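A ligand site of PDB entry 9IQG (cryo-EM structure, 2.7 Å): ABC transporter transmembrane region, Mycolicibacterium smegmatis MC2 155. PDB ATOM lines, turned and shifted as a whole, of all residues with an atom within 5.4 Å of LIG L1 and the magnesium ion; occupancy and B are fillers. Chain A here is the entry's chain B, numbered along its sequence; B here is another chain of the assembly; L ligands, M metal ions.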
ATOM      1  N   ASP A 166     -35.982  13.787  -6.580  1.00  0.00           N
ATOM      2  CA  ASP A 166     -34.730  13.153  -6.177  1.00  0.00           C
ATOM      3  C   ASP A 166     -34.791  12.664  -4.739  1.00  0.00           C
ATOM      4  O   ASP A 166     -34.206  11.616  -4.416  1.00  0.00           O
ATOM      5  CB  ASP A 166     -33.566  14.122  -6.354  1.00  0.00           C
ATOM      6  CG  ASP A 166     -33.300  14.463  -7.806  1.00  0.00           C
ATOM      7  OD1 ASP A 166     -33.984  13.886  -8.679  1.00  0.00           O
ATOM      8  OD2 ASP A 166     -32.418  15.295  -8.078  1.00  0.00           O
ATOM      9  N   TYR A 400     -25.949  21.963  -4.548  1.00  0.00           N
ATOM     10  CA  TYR A 400     -27.025  21.153  -3.976  1.00  0.00           C
ATOM     11  C   TYR A 400     -26.820  21.057  -2.471  1.00  0.00           C
ATOM     12  O   TYR A 400     -25.696  21.169  -1.976  1.00  0.00           O
ATOM     13  CB  TYR A 400     -27.031  19.750  -4.581  1.00  0.00           C
ATOM     14  CG  TYR A 400     -26.784  19.660  -6.067  1.00  0.00           C
ATOM     15  CD1 TYR A 400     -25.499  19.555  -6.581  1.00  0.00           C
ATOM     16  CD2 TYR A 400     -27.852  19.631  -6.965  1.00  0.00           C
ATOM     17  CE1 TYR A 400     -25.277  19.445  -7.932  1.00  0.00           C
ATOM     18  CE2 TYR A 400     -27.633  19.528  -8.322  1.00  0.00           C
ATOM     19  CZ  TYR A 400     -26.343  19.442  -8.799  1.00  0.00           C
ATOM     20  OH  TYR A 400     -26.121  19.332 -10.150  1.00  0.00           O
ATOM     21  N   VAL A 401     -27.918  20.835  -1.754  1.00  0.00           N
ATOM     22  CA  VAL A 401     -27.909  20.636  -0.296  1.00  0.00           C
ATOM     23  C   VAL A 401     -27.015  21.689   0.361  1.00  0.00           C
ATOM     24  O   VAL A 401     -25.871  21.401   0.760  1.00  0.00           O
ATOM     25  CB  VAL A 401     -27.587  19.169   0.058  1.00  0.00           C
ATOM     26  CG1 VAL A 401     -28.382  18.255  -0.857  1.00  0.00           C
ATOM     27  CG2 VAL A 401     -26.114  18.778  -0.103  1.00  0.00           C
ATOM     28  N   VAL A 406     -20.581  22.872  -5.029  1.00  0.00           N
ATOM     29  CA  VAL A 406     -20.155  21.993  -6.111  1.00  0.00           C
ATOM     30  C   VAL A 406     -19.585  22.835  -7.236  1.00  0.00           C
ATOM     31  O   VAL A 406     -18.759  22.360  -8.024  1.00  0.00           O
ATOM     32  CB  VAL A 406     -21.317  21.096  -6.601  1.00  0.00           C
ATOM     33  CG1 VAL A 406     -22.008  20.442  -5.420  1.00  0.00           C
ATOM     34  CG2 VAL A 406     -22.304  21.891  -7.429  1.00  0.00           C
ATOM     35  N   PRO A 425     -12.041  15.605 -14.119  1.00  0.00           N
ATOM     36  CA  PRO A 425     -12.236  14.401 -13.297  1.00  0.00           C
ATOM     37  C   PRO A 425     -13.691  13.952 -13.205  1.00  0.00           C
ATOM     38  O   PRO A 425     -14.601  14.599 -13.726  1.00  0.00           O
ATOM     39  CB  PRO A 425     -11.707  14.842 -11.924  1.00  0.00           C
ATOM     40  CG  PRO A 425     -10.704  15.881 -12.235  1.00  0.00           C
ATOM     41  CD  PRO A 425     -11.249  16.621 -13.423  1.00  0.00           C
ATOM     42  N   THR A 426     -13.900  12.825 -12.530  1.00  0.00           N
ATOM     43  CA  THR A 426     -15.177  12.139 -12.515  1.00  0.00           C
ATOM     44  C   THR A 426     -16.279  12.908 -11.814  1.00  0.00           C
ATOM     45  O   THR A 426     -17.438  12.815 -12.238  1.00  0.00           O
ATOM     46  CB  THR A 426     -14.988  10.765 -11.870  1.00  0.00           C
ATOM     47  OG1 THR A 426     -14.009  10.018 -12.599  1.00  0.00           O
ATOM     48  CG2 THR A 426     -16.273  10.002 -11.877  1.00  0.00           C
ATOM     49  N   GLY A 427     -15.984  13.675 -10.771  1.00  0.00           N
ATOM     50  CA  GLY A 427     -17.025  14.403 -10.083  1.00  0.00           C
ATOM     51  C   GLY A 427     -16.797  15.897 -10.097  1.00  0.00           C
ATOM     52  O   GLY A 427     -17.143  16.597  -9.137  1.00  0.00           O
ATOM     53  N   ALA A 428     -16.213  16.398 -11.181  1.00  0.00           N
ATOM     54  CA  ALA A 428     -15.806  17.801 -11.242  1.00  0.00           C
ATOM     55  C   ALA A 428     -17.012  18.735 -11.194  1.00  0.00           C
ATOM     56  O   ALA A 428     -16.980  19.758 -10.501  1.00  0.00           O
ATOM     57  CB  ALA A 428     -14.973  18.048 -12.490  1.00  0.00           C
ATOM     58  N   GLY A 429     -18.067  18.421 -11.932  1.00  0.00           N
ATOM     59  CA  GLY A 429     -19.202  19.319 -12.043  1.00  0.00           C
ATOM     60  C   GLY A 429     -19.594  19.609 -13.469  1.00  0.00           C
ATOM     61  O   GLY A 429     -20.279  20.585 -13.750  1.00  0.00           O
ATOM     62  N   LYS A 430     -19.152  18.744 -14.394  1.00  0.00           N
ATOM     63  CA  LYS A 430     -19.448  18.935 -15.806  1.00  0.00           C
ATOM     64  C   LYS A 430     -20.934  18.815 -16.106  1.00  0.00           C
ATOM     65  O   LYS A 430     -21.475  19.607 -16.873  1.00  0.00           O
ATOM     66  CB  LYS A 430     -18.652  17.938 -16.635  1.00  0.00           C
ATOM     67  CG  LYS A 430     -17.148  17.967 -16.371  1.00  0.00           C
ATOM     68  CD  LYS A 430     -16.406  16.957 -17.222  1.00  0.00           C
ATOM     69  CE  LYS A 430     -16.896  15.551 -16.960  1.00  0.00           C
ATOM     70  NZ  LYS A 430     -16.531  15.087 -15.600  1.00  0.00           N
ATOM     71  N   THR A 431     -21.612  17.826 -15.514  1.00  0.00           N
ATOM     72  CA  THR A 431     -23.054  17.715 -15.692  1.00  0.00           C
ATOM     73  C   THR A 431     -23.794  18.853 -15.000  1.00  0.00           C
ATOM     74  O   THR A 431     -24.806  19.344 -15.511  1.00  0.00           O
ATOM     75  CB  THR A 431     -23.548  16.362 -15.170  1.00  0.00           C
ATOM     76  OG1 THR A 431     -22.785  15.304 -15.760  1.00  0.00           O
ATOM     77  CG2 THR A 431     -25.019  16.159 -15.511  1.00  0.00           C
ATOM     78  N   THR A 432     -23.311  19.260 -13.825  1.00  0.00           N
ATOM     79  CA  THR A 432     -23.939  20.368 -13.107  1.00  0.00           C
ATOM     80  C   THR A 432     -23.894  21.657 -13.918  1.00  0.00           C
ATOM     81  O   THR A 432     -24.838  22.442 -13.880  1.00  0.00           O
ATOM     82  CB  THR A 432     -23.262  20.562 -11.758  1.00  0.00           C
ATOM     83  OG1 THR A 432     -23.409  19.374 -10.974  1.00  0.00           O
ATOM     84  CG2 THR A 432     -23.867  21.733 -11.009  1.00  0.00           C
ATOM     85  N   LEU A 433     -22.817  21.874 -14.680  1.00  0.00           N
ATOM     86  CA  LEU A 433     -22.694  23.091 -15.467  1.00  0.00           C
ATOM     87  C   LEU A 433     -23.775  23.175 -16.534  1.00  0.00           C
ATOM     88  O   LEU A 433     -24.454  24.201 -16.676  1.00  0.00           O
ATOM     89  CB  LEU A 433     -21.302  23.147 -16.101  1.00  0.00           C
ATOM     90  CG  LEU A 433     -20.859  24.508 -16.639  1.00  0.00           C
ATOM     91  CD1 LEU A 433     -20.372  25.362 -15.485  1.00  0.00           C
ATOM     92  CD2 LEU A 433     -19.779  24.348 -17.676  1.00  0.00           C
ATOM     93  N   TYR A 441     -31.670  23.539 -12.328  1.00  0.00           N
ATOM     94  CA  TYR A 441     -31.557  24.031 -10.973  1.00  0.00           C
ATOM     95  C   TYR A 441     -31.267  25.519 -11.023  1.00  0.00           C
ATOM     96  O   TYR A 441     -30.751  26.044 -12.013  1.00  0.00           O
ATOM     97  CB  TYR A 441     -30.461  23.308 -10.191  1.00  0.00           C
ATOM     98  CG  TYR A 441     -30.580  21.800 -10.181  1.00  0.00           C
ATOM     99  CD1 TYR A 441     -29.990  21.030 -11.162  1.00  0.00           C
ATOM    100  CD2 TYR A 441     -31.281  21.154  -9.166  1.00  0.00           C
ATOM    101  CE1 TYR A 441     -30.104  19.656 -11.156  1.00  0.00           C
ATOM    102  CE2 TYR A 441     -31.401  19.787  -9.150  1.00  0.00           C
ATOM    103  CZ  TYR A 441     -30.808  19.046 -10.146  1.00  0.00           C
ATOM    104  OH  TYR A 441     -30.921  17.672 -10.141  1.00  0.00           O
ATOM    105  N   GLN A 472     -27.104  12.521 -20.098  1.00  0.00           N
ATOM    106  CA  GLN A 472     -26.112  11.513 -19.725  1.00  0.00           C
ATOM    107  C   GLN A 472     -26.785  10.182 -19.400  1.00  0.00           C
ATOM    108  O   GLN A 472     -26.263   9.122 -19.748  1.00  0.00           O
ATOM    109  CB  GLN A 472     -25.285  11.997 -18.540  1.00  0.00           C
ATOM    110  CG  GLN A 472     -23.872  11.458 -18.525  1.00  0.00           C
ATOM    111  CD  GLN A 472     -23.307  11.296 -17.125  1.00  0.00           C
ATOM    112  OE1 GLN A 472     -23.534  12.142 -16.260  1.00  0.00           O
ATOM    113  NE2 GLN A 472     -22.588  10.209 -16.896  1.00  0.00           N
ATOM    114  N   ASP A 552     -24.036  15.623 -23.530  1.00  0.00           N
ATOM    115  CA  ASP A 552     -23.450  15.275 -22.234  1.00  0.00           C
ATOM    116  C   ASP A 552     -23.096  13.797 -22.268  1.00  0.00           C
ATOM    117  O   ASP A 552     -23.906  12.939 -21.913  1.00  0.00           O
ATOM    118  CB  ASP A 552     -24.416  15.622 -21.108  1.00  0.00           C
ATOM    119  CG  ASP A 552     -23.815  15.390 -19.728  1.00  0.00           C
ATOM    120  OD1 ASP A 552     -22.578  15.292 -19.621  1.00  0.00           O
ATOM    121  OD2 ASP A 552     -24.588  15.312 -18.749  1.00  0.00           O
ATOM    122  N   GLU A 553     -21.863  13.503 -22.688  1.00  0.00           N
ATOM    123  CA  GLU A 553     -21.357  12.128 -22.818  1.00  0.00           C
ATOM    124  C   GLU A 553     -22.264  11.306 -23.732  1.00  0.00           C
ATOM    125  O   GLU A 553     -22.843  10.291 -23.335  1.00  0.00           O
ATOM    126  CB  GLU A 553     -21.200  11.486 -21.440  1.00  0.00           C
ATOM    127  CG  GLU A 553     -19.826  11.670 -20.830  1.00  0.00           C
ATOM    128  CD  GLU A 553     -19.779  11.273 -19.368  1.00  0.00           C
ATOM    129  OE1 GLU A 553     -19.788  12.176 -18.506  1.00  0.00           O
ATOM    130  OE2 GLU A 553     -19.727  10.057 -19.089  1.00  0.00           O
ATOM    131  N   ARG B 217     -37.105  14.493 -16.368  1.00  0.00           N
ATOM    132  CA  ARG B 217     -35.922  15.221 -16.828  1.00  0.00           C
ATOM    133  C   ARG B 217     -35.879  15.310 -18.346  1.00  0.00           C
ATOM    134  O   ARG B 217     -35.527  16.346 -18.903  1.00  0.00           O
ATOM    135  CB  ARG B 217     -34.657  14.545 -16.301  1.00  0.00           C
ATOM    136  CG  ARG B 217     -34.294  14.970 -14.883  1.00  0.00           C
ATOM    137  CD  ARG B 217     -33.080  14.217 -14.375  1.00  0.00           C
ATOM    138  NE  ARG B 217     -32.509  14.858 -13.191  1.00  0.00           N
ATOM    139  CZ  ARG B 217     -32.953  14.676 -11.954  1.00  0.00           C
ATOM    140  NH1 ARG B 217     -33.973  13.886 -11.694  1.00  0.00           N
ATOM    141  NH2 ARG B 217     -32.346  15.310 -10.957  1.00  0.00           N
ATOM    142  N   ILE B 482     -29.087   8.956  -8.203  1.00  0.00           N
ATOM    143  CA  ILE B 482     -29.057  10.161  -9.026  1.00  0.00           C
ATOM    144  C   ILE B 482     -28.564  11.387  -8.278  1.00  0.00           C
ATOM    145  O   ILE B 482     -28.359  12.441  -8.893  1.00  0.00           O
ATOM    146  CB  ILE B 482     -30.436  10.438  -9.652  1.00  0.00           C
ATOM    147  CG1 ILE B 482     -31.573  10.091  -8.690  1.00  0.00           C
ATOM    148  CG2 ILE B 482     -30.599   9.682 -10.958  1.00  0.00           C
ATOM    149  CD1 ILE B 482     -31.755  11.046  -7.552  1.00  0.00           C
ATOM    150  N   ASN B 483     -28.367  11.286  -6.957  1.00  0.00           N
ATOM    151  CA  ASN B 483     -27.660  12.313  -6.207  1.00  0.00           C
ATOM    152  C   ASN B 483     -26.148  12.168  -6.320  1.00  0.00           C
ATOM    153  O   ASN B 483     -25.421  12.814  -5.565  1.00  0.00           O
ATOM    154  CB  ASN B 483     -28.089  12.276  -4.737  1.00  0.00           C
ATOM    155  CG  ASN B 483     -27.656  11.006  -4.035  1.00  0.00           C
ATOM    156  OD1 ASN B 483     -27.838   9.904  -4.553  1.00  0.00           O
ATOM    157  ND2 ASN B 483     -27.094  11.158  -2.845  1.00  0.00           N
ATOM    158  N   PHE B 484     -25.683  11.331  -7.240  1.00  0.00           N
ATOM    159  CA  PHE B 484     -24.286  11.160  -7.559  1.00  0.00           C
ATOM    160  C   PHE B 484     -24.062  11.424  -9.034  1.00  0.00           C
ATOM    161  O   PHE B 484     -24.999  11.432  -9.835  1.00  0.00           O
ATOM    162  CB  PHE B 484     -23.792   9.743  -7.210  1.00  0.00           C
ATOM    163  CG  PHE B 484     -23.744   9.458  -5.743  1.00  0.00           C
ATOM    164  CD1 PHE B 484     -22.827  10.101  -4.935  1.00  0.00           C
ATOM    165  CD2 PHE B 484     -24.608   8.542  -5.171  1.00  0.00           C
ATOM    166  CE1 PHE B 484     -22.775   9.835  -3.578  1.00  0.00           C
ATOM    167  CE2 PHE B 484     -24.559   8.269  -3.821  1.00  0.00           C
ATOM    168  CZ  PHE B 484     -23.637   8.919  -3.023  1.00  0.00           C
ATOM    169  N   SER B 485     -22.806  11.659  -9.402  1.00  0.00           N
ATOM    170  CA  SER B 485     -22.457  11.721 -10.804  1.00  0.00           C
ATOM    171  C   SER B 485     -22.427  10.311 -11.402  1.00  0.00           C
ATOM    172  O   SER B 485     -22.410   9.309 -10.685  1.00  0.00           O
ATOM    173  CB  SER B 485     -21.115  12.415 -10.989  1.00  0.00           C
ATOM    174  OG  SER B 485     -20.044  11.563 -10.629  1.00  0.00           O
ATOM    175  N   GLY B 486     -22.450  10.243 -12.733  1.00  0.00           N
ATOM    176  CA  GLY B 486     -22.473   8.949 -13.395  1.00  0.00           C
ATOM    177  C   GLY B 486     -21.257   8.106 -13.078  1.00  0.00           C
ATOM    178  O   GLY B 486     -21.368   6.905 -12.817  1.00  0.00           O
ATOM    179  N   GLN B 488     -19.396   8.487 -10.402  1.00  0.00           N
ATOM    180  CA  GLN B 488     -19.493   8.127  -8.989  1.00  0.00           C
ATOM    181  C   GLN B 488     -20.365   6.896  -8.809  1.00  0.00           C
ATOM    182  O   GLN B 488     -20.045   6.010  -8.000  1.00  0.00           O
ATOM    183  CB  GLN B 488     -20.047   9.302  -8.177  1.00  0.00           C
ATOM    184  CG  GLN B 488     -18.990  10.301  -7.744  1.00  0.00           C
ATOM    185  CD  GLN B 488     -19.575  11.510  -7.072  1.00  0.00           C
ATOM    186  OE1 GLN B 488     -20.790  11.717  -7.076  1.00  0.00           O
ATOM    187  NE2 GLN B 488     -18.719  12.340  -6.485  1.00  0.00           N
HETATM  188  P1  LIG L   1     -19.450  15.670 -13.058  1.00  0.00           P
HETATM  189  O1  LIG L   1     -19.606  14.216 -12.834  1.00  0.00           O
HETATM  190  O2  LIG L   1     -18.010  16.091 -13.160  1.00  0.00           O
HETATM  191  O3  LIG L   1     -20.280  16.153 -14.205  1.00  0.00           O
HETATM  192  P2  LIG L   1     -21.581  16.670 -11.324  1.00  0.00           P
HETATM  193  O4  LIG L   1     -22.200  17.449 -12.430  1.00  0.00           O
HETATM  194  O5  LIG L   1     -22.267  15.413 -10.904  1.00  0.00           O
HETATM  195  O6  LIG L   1     -20.072  16.333 -11.717  1.00  0.00           O
HETATM  196  O7  LIG L   1     -21.394  17.625 -10.052  1.00  0.00           O
HETATM  197  C1  LIG L   1     -20.445  17.253  -9.023  1.00  0.00           C
HETATM  198  C2  LIG L   1     -21.181  16.677  -7.842  1.00  0.00           C
HETATM  199  O8  LIG L   1     -22.591  16.974  -7.955  1.00  0.00           O
HETATM  200  C3  LIG L   1     -21.086  15.155  -7.674  1.00  0.00           C
HETATM  201  O9  LIG L   1     -20.304  14.813  -6.529  1.00  0.00           O
HETATM  202  C4  LIG L   1     -22.539  14.669  -7.530  1.00  0.00           C
HETATM  203  O10 LIG L   1     -22.710  13.785  -6.449  1.00  0.00           O
HETATM  204  C5  LIG L   1     -23.315  15.968  -7.296  1.00  0.00           C
HETATM  205  N1  LIG L   1     -24.665  15.937  -7.848  1.00  0.00           N
HETATM  206  C6  LIG L   1     -25.004  15.883  -9.173  1.00  0.00           C
HETATM  207  N2  LIG L   1     -26.304  15.865  -9.374  1.00  0.00           N
HETATM  208  C7  LIG L   1     -26.848  15.915  -8.104  1.00  0.00           C
HETATM  209  C8  LIG L   1     -28.174  15.924  -7.638  1.00  0.00           C
HETATM  210  N3  LIG L   1     -29.235  15.890  -8.447  1.00  0.00           N
HETATM  211  N4  LIG L   1     -28.378  15.977  -6.298  1.00  0.00           N
HETATM  212  C9  LIG L   1     -27.311  16.019  -5.500  1.00  0.00           C
HETATM  213  N5  LIG L   1     -26.017  16.011  -5.819  1.00  0.00           N
HETATM  214  C10 LIG L   1     -25.850  15.956  -7.142  1.00  0.00           C
HETATM  215  V1  LG2 L   2     -19.207  11.971 -14.876  1.00  0.00           V
HETATM  216  O1  LG2 L   2     -17.605  12.990 -15.056  1.00  0.00           O
HETATM  217  O2  LG2 L   2     -19.258  10.645 -16.250  1.00  0.00           O
HETATM  218  O3  LG2 L   2     -19.253  11.103 -13.182  1.00  0.00           O
HETATM  219  O4  LG2 L   2     -20.726  13.112 -15.049  1.00  0.00           O
HETATM  220 MG    MG M   1     -22.639  13.505 -15.083  1.00  0.00          MG
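An oxygen (O3) of LIG L1 lies within hydrogen-bond range of the backbone NH (N) of Thr 431, at 2.5 Å.
An oxygen (O2) of LIG L1 is in hydrogen-bond range of the backbone NH (N) of Ala 428.
OH of Tyr 441 sits at hydrogen-bond distance from N3 of LIG L1 (3.0 Å).
N of Thr 432 lies within hydrogen-bond range of O4 of LIG L1, 2.5 Å away.
A nitrogen (N3) of LIG L1 sits at hydrogen-bond distance from the side-chain carboxylate (OD2) of Asp 166, at 3.3 Å.
O1 of LG2 L2 lies close to NZ of Lys 430.
The side-chain amino group (NZ) of Lys 430 lies within salt-bridge range of an oxygen (O2) of LIG L1 (3.0 Å).
The backbone NH (N) of Gly 429 sits at hydrogen-bond distance from an oxygen (O2) of LIG L1, 2.6 Å away.
OE1 of Gln 488 of chain B lies within hydrogen-bond range of O10 of LIG L1 (2.9 Å).
The backbone carbonyl oxygen (O) of Thr 426 sits close to an oxygen (O1) of LIG L1 (2.6 Å).
The side-chain hydroxyl of Ser 485 of chain B sits close to an oxygen (O3) of LG2 L2, 2.7 Å away.
An oxygen (O3) of LIG L1 is in hydrogen-bond range of the backbone NH (N) of Lys 430 (2.8 Å).
The side-chain hydroxyl (OG) of Ser 485 of chain B sits close to an oxygen (O1) of LIG L1, at 3.5 Å.
OG1 of Thr 431 sits close to O3 of LIG L1 (3.1 Å).
O10 of LIG L1 lies within hydrogen-bond range of O of Asn 483 of chain B, 3.0 Å away.
O3 of LG2 L2 lies close to O of Thr 426 (2.7 Å).
An oxygen (O4) of LIG L1 is in hydrogen-bond range of the side-chain hydroxyl of Thr 432 (2.7 Å).
An oxygen (O4) of LG2 L2 lies close to an oxygen (O1) of LIG L1, 2.7 Å away.
OH of Tyr 441 lies within hydrogen-bond range of OD2 of Asp 166, 3.5 Å away.
NH2 of Arg 217 of chain B is in hydrogen-bond range of OH of Tyr 441 (2.9 Å).
O of Thr 426 lies within hydrogen-bond range of OG of Ser 485 of chain B (3.3 Å).
The side-chain hydroxyl of Tyr 400 sits at hydrogen-bond distance from the side-chain hydroxyl of Thr 432 (2.8 Å).
The backbone NH (N) of Ser 485 of chain B lies within hydrogen-bond range of the side-chain amide oxygen (OE1) of Gln 488 of chain B.
The side-chain amino group (NZ) of Lys 430 is in hydrogen-bond range of the backbone carbonyl oxygen (O) of Pro 425 (2.7 Å).
The side-chain carboxylate of Asp 552 lies close to the side-chain hydroxyl of Thr 431.
OD2 of Asp 166 is in salt-bridge range of NH2 of Arg 217 of chain B (2.9 Å).
Tyr 400 touches LIG L1.
Pro 425 touches LIG L1 (O to O2, 3.8 Å).
Gly 427 touches LIG L1 (C to O2, 3.3 Å).
Ile 482 of chain B touches LIG L1 (O to N3, 3.6 Å).
Phe 484 of chain B touches LIG L1 (CA to O10, 3.3 Å).
Hydrophobic or aromatic side chains within 4 Å of LIG L1: Tyr 400, Ala 428, Tyr 441 and Phe 484 of chain B.
The nearest printed residue that does not touch LIG L1 is Arg 217 of chain B (4.04 Å).
Of the 24 residues printed, 2 come within 4 Å of the magnesium ion.
The magnesium ion is bound by the side-chain hydroxyl of Thr 431 (1.9 Å), an oxygen (O4) of LG2 L2 (2.0 Å) and the side-chain amide oxygen of Gln 472 (2.0 Å).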
